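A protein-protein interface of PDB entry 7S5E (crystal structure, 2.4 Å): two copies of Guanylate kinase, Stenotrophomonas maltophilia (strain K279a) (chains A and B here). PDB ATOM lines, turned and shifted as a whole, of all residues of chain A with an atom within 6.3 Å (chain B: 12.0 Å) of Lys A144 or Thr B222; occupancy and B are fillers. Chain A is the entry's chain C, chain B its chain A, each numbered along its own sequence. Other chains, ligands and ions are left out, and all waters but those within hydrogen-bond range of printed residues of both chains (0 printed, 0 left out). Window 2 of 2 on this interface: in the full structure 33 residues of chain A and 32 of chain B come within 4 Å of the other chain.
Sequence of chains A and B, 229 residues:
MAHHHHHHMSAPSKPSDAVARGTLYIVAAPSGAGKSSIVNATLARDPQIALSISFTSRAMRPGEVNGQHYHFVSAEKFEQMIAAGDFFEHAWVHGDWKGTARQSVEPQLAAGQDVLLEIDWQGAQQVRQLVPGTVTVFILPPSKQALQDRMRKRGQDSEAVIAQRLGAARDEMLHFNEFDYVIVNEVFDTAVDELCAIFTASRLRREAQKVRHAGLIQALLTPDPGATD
The side-chain amino group (NZ) of Lys A144 sits close to the backbone carbonyl oxygen (O) of Ala B219, at 3.4 Å.
No position is printed for both chains.
N of Ala A146 sits at hydrogen-bond distance from OG of Ser A143 (3.1 Å).
Among the printed residues, merely in contact across the chains: Pro A142 with Leu B216, Ser A143 with Leu B216, Lys A144 with Leu B220, Pro A141 with Leu B216, Lys A144 with Thr B222, Arg A170 with Leu B221, Pro A141 with Leu B220 and Ser A143 with Leu B220.
Printed residues of chain A that touch a printed residue of chain B: Pro A141, Pro A142, Ser A143, Lys A144 and Arg A170.
Among the printed residues, no Asp or Glu carboxylate lies within 4 Å of a Lys or Arg side-chain nitrogen of the other chain.
Pro A142 touches one residue of chain B.
Ser A143 touches two residues of chain B.
Lys A144 touches just these residues of chain B: Ala B219, Leu B220 and Thr B222.
No residue of chain B comes within 4 Å of Gln A145.
No residue of chain B comes within 4 Å of Ala A146.
Leu A166 touches none of the printed residues of chain B.
Arg A170 touches just one residue of chain B: Leu B221 (3.9 Å).
Ala B214 touches none of the printed residues of chain A.
Printed residues of chain A within 4 Å of Leu B216: Pro A141 (3.6 Å), Pro A142 (3.3 Å) and Ser A143 (3.5 Å).
Of the printed residues of chain A, Ala B219 touches Lys A144.
Of the printed residues of chain A, Leu B220 touches Pro A141, Ser A143 and Lys A144.
Of the printed residues of chain A, Leu B221 touches Arg A170 (3.9 Å).
Of chain A, only Lys A144 comes within 4 Å of Thr B222.
The nearest printed residue of chain A that does not touch Leu B221 is Lys A144 (5.4 Å).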
ATOM      1  N   PRO A 141       1.024 -25.130  -8.677  1.00  0.00           N
ATOM      2  CA  PRO A 141       0.007 -25.302  -7.645  1.00  0.00           C
ATOM      3  C   PRO A 141      -1.108 -24.291  -7.834  1.00  0.00           C
ATOM      4  O   PRO A 141      -0.900 -23.241  -8.458  1.00  0.00           O
ATOM      5  CB  PRO A 141       0.782 -25.048  -6.345  1.00  0.00           C
ATOM      6  CG  PRO A 141       1.870 -24.123  -6.751  1.00  0.00           C
ATOM      7  CD  PRO A 141       2.268 -24.549  -8.139  1.00  0.00           C
ATOM      8  N   PRO A 142      -2.306 -24.566  -7.313  1.00  0.00           N
ATOM      9  CA  PRO A 142      -3.438 -23.658  -7.560  1.00  0.00           C
ATOM     10  C   PRO A 142      -3.375 -22.348  -6.786  1.00  0.00           C
ATOM     11  O   PRO A 142      -4.155 -21.438  -7.098  1.00  0.00           O
ATOM     12  CB  PRO A 142      -4.648 -24.491  -7.123  1.00  0.00           C
ATOM     13  CG  PRO A 142      -4.099 -25.409  -6.074  1.00  0.00           C
ATOM     14  CD  PRO A 142      -2.686 -25.725  -6.486  1.00  0.00           C
ATOM     15  N   SER A 143      -2.469 -22.208  -5.820  1.00  0.00           N
ATOM     16  CA  SER A 143      -2.322 -20.963  -5.073  1.00  0.00           C
ATOM     17  C   SER A 143      -1.041 -21.039  -4.259  1.00  0.00           C
ATOM     18  O   SER A 143      -0.532 -22.126  -3.968  1.00  0.00           O
ATOM     19  CB  SER A 143      -3.517 -20.690  -4.148  1.00  0.00           C
ATOM     20  OG  SER A 143      -3.594 -21.640  -3.098  1.00  0.00           O
ATOM     21  N   LYS A 144      -0.531 -19.860  -3.897  1.00  0.00           N
ATOM     22  CA  LYS A 144       0.660 -19.794  -3.058  1.00  0.00           C
ATOM     23  C   LYS A 144       0.398 -20.389  -1.684  1.00  0.00           C
ATOM     24  O   LYS A 144       1.294 -21.003  -1.093  1.00  0.00           O
ATOM     25  CB  LYS A 144       1.152 -18.350  -2.938  1.00  0.00           C
ATOM     26  CG  LYS A 144       2.601 -18.235  -2.482  1.00  0.00           C
ATOM     27  CD  LYS A 144       3.170 -16.852  -2.748  1.00  0.00           C
ATOM     28  CE  LYS A 144       4.658 -16.798  -2.439  1.00  0.00           C
ATOM     29  NZ  LYS A 144       5.218 -15.438  -2.684  1.00  0.00           N
ATOM     30  N   GLN A 145      -0.821 -20.227  -1.161  1.00  0.00           N
ATOM     31  CA  GLN A 145      -1.141 -20.803   0.140  1.00  0.00           C
ATOM     32  C   GLN A 145      -1.150 -22.324   0.074  1.00  0.00           C
ATOM     33  O   GLN A 145      -0.781 -22.995   1.044  1.00  0.00           O
ATOM     34  CB  GLN A 145      -2.488 -20.277   0.634  1.00  0.00           C
ATOM     35  N   ALA A 146      -1.591 -22.888  -1.054  1.00  0.00           N
ATOM     36  CA  ALA A 146      -1.573 -24.340  -1.202  1.00  0.00           C
ATOM     37  C   ALA A 146      -0.152 -24.884  -1.149  1.00  0.00           C
ATOM     38  O   ALA A 146       0.088 -25.965  -0.598  1.00  0.00           O
ATOM     39  CB  ALA A 146      -2.253 -24.741  -2.511  1.00  0.00           C
ATOM     40  N   LEU A 147       0.809 -24.147  -1.714  1.00  0.00           N
ATOM     41  CA  LEU A 147       2.202 -24.578  -1.654  1.00  0.00           C
ATOM     42  C   LEU A 147       2.720 -24.560  -0.217  1.00  0.00           C
ATOM     43  O   LEU A 147       3.321 -25.536   0.250  1.00  0.00           O
ATOM     44  CB  LEU A 147       3.064 -23.701  -2.567  1.00  0.00           C
ATOM     45  N   GLN A 148       2.481 -23.458   0.506  1.00  0.00           N
ATOM     46  CA  GLN A 148       2.983 -23.335   1.874  1.00  0.00           C
ATOM     47  C   GLN A 148       2.383 -24.388   2.798  1.00  0.00           C
ATOM     48  O   GLN A 148       2.997 -24.740   3.811  1.00  0.00           O
ATOM     49  CB  GLN A 148       2.704 -21.932   2.418  1.00  0.00           C
ATOM     50  N   ASP A 149       1.189 -24.899   2.476  1.00  0.00           N
ATOM     51  CA  ASP A 149       0.646 -26.019   3.241  1.00  0.00           C
ATOM     52  C   ASP A 149       1.448 -27.290   2.987  1.00  0.00           C
ATOM     53  O   ASP A 149       1.765 -28.031   3.926  1.00  0.00           O
ATOM     54  CB  ASP A 149      -0.828 -26.230   2.892  1.00  0.00           C
ATOM     55  N   LEU A 166      10.430 -23.068   0.366  1.00  0.00           N
ATOM     56  CA  LEU A 166       9.593 -22.213  -0.473  1.00  0.00           C
ATOM     57  C   LEU A 166      10.446 -21.442  -1.475  1.00  0.00           C
ATOM     58  O   LEU A 166      10.035 -21.236  -2.622  1.00  0.00           O
ATOM     59  CB  LEU A 166       8.756 -21.258   0.385  1.00  0.00           C
ATOM     60  CG  LEU A 166       7.550 -20.584  -0.297  1.00  0.00           C
ATOM     61  CD1 LEU A 166       6.471 -20.255   0.728  1.00  0.00           C
ATOM     62  CD2 LEU A 166       7.918 -19.330  -1.085  1.00  0.00           C
ATOM     63  N   ARG A 170       9.907 -21.196  -5.389  1.00  0.00           N
ATOM     64  CA  ARG A 170       9.804 -19.968  -6.170  1.00  0.00           C
ATOM     65  C   ARG A 170      10.870 -19.913  -7.262  1.00  0.00           C
ATOM     66  O   ARG A 170      10.587 -19.517  -8.400  1.00  0.00           O
ATOM     67  CB  ARG A 170       9.910 -18.752  -5.246  1.00  0.00           C
ATOM     68  N   HIS B 213      -4.106 -17.385 -16.017  1.00  0.00           N
ATOM     69  CA  HIS B 213      -3.685 -17.423 -14.620  1.00  0.00           C
ATOM     70  C   HIS B 213      -2.704 -16.305 -14.285  1.00  0.00           C
ATOM     71  O   HIS B 213      -1.771 -16.493 -13.498  1.00  0.00           O
ATOM     72  CB  HIS B 213      -3.078 -18.780 -14.268  1.00  0.00           C
ATOM     73  CG  HIS B 213      -4.016 -19.930 -14.456  1.00  0.00           C
ATOM     74  ND1 HIS B 213      -4.082 -20.657 -15.628  1.00  0.00           N
ATOM     75  CD2 HIS B 213      -4.929 -20.480 -13.622  1.00  0.00           C
ATOM     76  CE1 HIS B 213      -4.994 -21.604 -15.505  1.00  0.00           C
ATOM     77  NE2 HIS B 213      -5.525 -21.515 -14.299  1.00  0.00           N
ATOM     78  N   ALA B 214      -2.910 -15.121 -14.867  1.00  0.00           N
ATOM     79  CA  ALA B 214      -1.975 -14.019 -14.656  1.00  0.00           C
ATOM     80  C   ALA B 214      -1.827 -13.697 -13.176  1.00  0.00           C
ATOM     81  O   ALA B 214      -0.710 -13.534 -12.673  1.00  0.00           O
ATOM     82  CB  ALA B 214      -2.434 -12.783 -15.429  1.00  0.00           C
ATOM     83  N   GLY B 215      -2.951 -13.601 -12.460  1.00  0.00           N
ATOM     84  CA  GLY B 215      -2.885 -13.275 -11.043  1.00  0.00           C
ATOM     85  C   GLY B 215      -2.245 -14.370 -10.209  1.00  0.00           C
ATOM     86  O   GLY B 215      -1.428 -14.091  -9.328  1.00  0.00           O
ATOM     87  N   LEU B 216      -2.607 -15.628 -10.471  1.00  0.00           N
ATOM     88  CA  LEU B 216      -2.001 -16.734  -9.737  1.00  0.00           C
ATOM     89  C   LEU B 216      -0.496 -16.772  -9.965  1.00  0.00           C
ATOM     90  O   LEU B 216       0.281 -16.946  -9.018  1.00  0.00           O
ATOM     91  CB  LEU B 216      -2.640 -18.057 -10.156  1.00  0.00           C
ATOM     92  CG  LEU B 216      -1.912 -19.325  -9.707  1.00  0.00           C
ATOM     93  CD1 LEU B 216      -1.848 -19.386  -8.195  1.00  0.00           C
ATOM     94  CD2 LEU B 216      -2.576 -20.574 -10.272  1.00  0.00           C
ATOM     95  N   ILE B 217      -0.067 -16.586 -11.214  1.00  0.00           N
ATOM     96  CA  ILE B 217       1.357 -16.624 -11.523  1.00  0.00           C
ATOM     97  C   ILE B 217       2.064 -15.435 -10.887  1.00  0.00           C
ATOM     98  O   ILE B 217       3.167 -15.569 -10.338  1.00  0.00           O
ATOM     99  CB  ILE B 217       1.565 -16.681 -13.048  1.00  0.00           C
ATOM    100  CG1 ILE B 217       1.030 -17.999 -13.608  1.00  0.00           C
ATOM    101  CG2 ILE B 217       3.027 -16.531 -13.407  1.00  0.00           C
ATOM    102  CD1 ILE B 217       1.074 -18.078 -15.115  1.00  0.00           C
ATOM    103  N   GLN B 218       1.431 -14.257 -10.925  1.00  0.00           N
ATOM    104  CA  GLN B 218       2.010 -13.085 -10.274  1.00  0.00           C
ATOM    105  C   GLN B 218       2.212 -13.339  -8.786  1.00  0.00           C
ATOM    106  O   GLN B 218       3.234 -12.944  -8.210  1.00  0.00           O
ATOM    107  CB  GLN B 218       1.120 -11.859 -10.498  1.00  0.00           C
ATOM    108  N   ALA B 219       1.247 -14.009  -8.150  1.00  0.00           N
ATOM    109  CA  ALA B 219       1.364 -14.322  -6.732  1.00  0.00           C
ATOM    110  C   ALA B 219       2.494 -15.313  -6.461  1.00  0.00           C
ATOM    111  O   ALA B 219       3.256 -15.148  -5.500  1.00  0.00           O
ATOM    112  CB  ALA B 219       0.034 -14.872  -6.215  1.00  0.00           C
ATOM    113  N   LEU B 220       2.624 -16.347  -7.297  1.00  0.00           N
ATOM    114  CA  LEU B 220       3.617 -17.381  -7.031  1.00  0.00           C
ATOM    115  C   LEU B 220       5.051 -16.885  -7.196  1.00  0.00           C
ATOM    116  O   LEU B 220       5.959 -17.401  -6.533  1.00  0.00           O
ATOM    117  CB  LEU B 220       3.368 -18.580  -7.945  1.00  0.00           C
ATOM    118  CG  LEU B 220       2.116 -19.416  -7.675  1.00  0.00           C
ATOM    119  CD1 LEU B 220       1.918 -20.461  -8.771  1.00  0.00           C
ATOM    120  CD2 LEU B 220       2.214 -20.085  -6.327  1.00  0.00           C
ATOM    121  N   LEU B 221       5.285 -15.889  -8.052  1.00  0.00           N
ATOM    122  CA  LEU B 221       6.650 -15.465  -8.338  1.00  0.00           C
ATOM    123  C   LEU B 221       7.112 -14.246  -7.546  1.00  0.00           C
ATOM    124  O   LEU B 221       8.300 -13.907  -7.607  1.00  0.00           O
ATOM    125  CB  LEU B 221       6.803 -15.186  -9.836  1.00  0.00           C
ATOM    126  CG  LEU B 221       6.752 -16.469 -10.667  1.00  0.00           C
ATOM    127  CD1 LEU B 221       7.056 -16.194 -12.136  1.00  0.00           C
ATOM    128  CD2 LEU B 221       7.679 -17.536 -10.094  1.00  0.00           C
ATOM    129  N   THR B 222       6.229 -13.591  -6.801  1.00  0.00           N
ATOM    130  CA  THR B 222       6.633 -12.425  -6.025  1.00  0.00           C
ATOM    131  C   THR B 222       7.083 -12.835  -4.628  1.00  0.00           C
ATOM    132  O   THR B 222       7.974 -13.671  -4.474  1.00  0.00           O
ATOM    133  CB  THR B 222       5.497 -11.394  -5.910  1.00  0.00           C
ATOM    134  OG1 THR B 222       5.913 -10.316  -5.061  1.00  0.00           O
ATOM    135  CG2 THR B 222       4.254 -12.033  -5.324  1.00  0.00           C
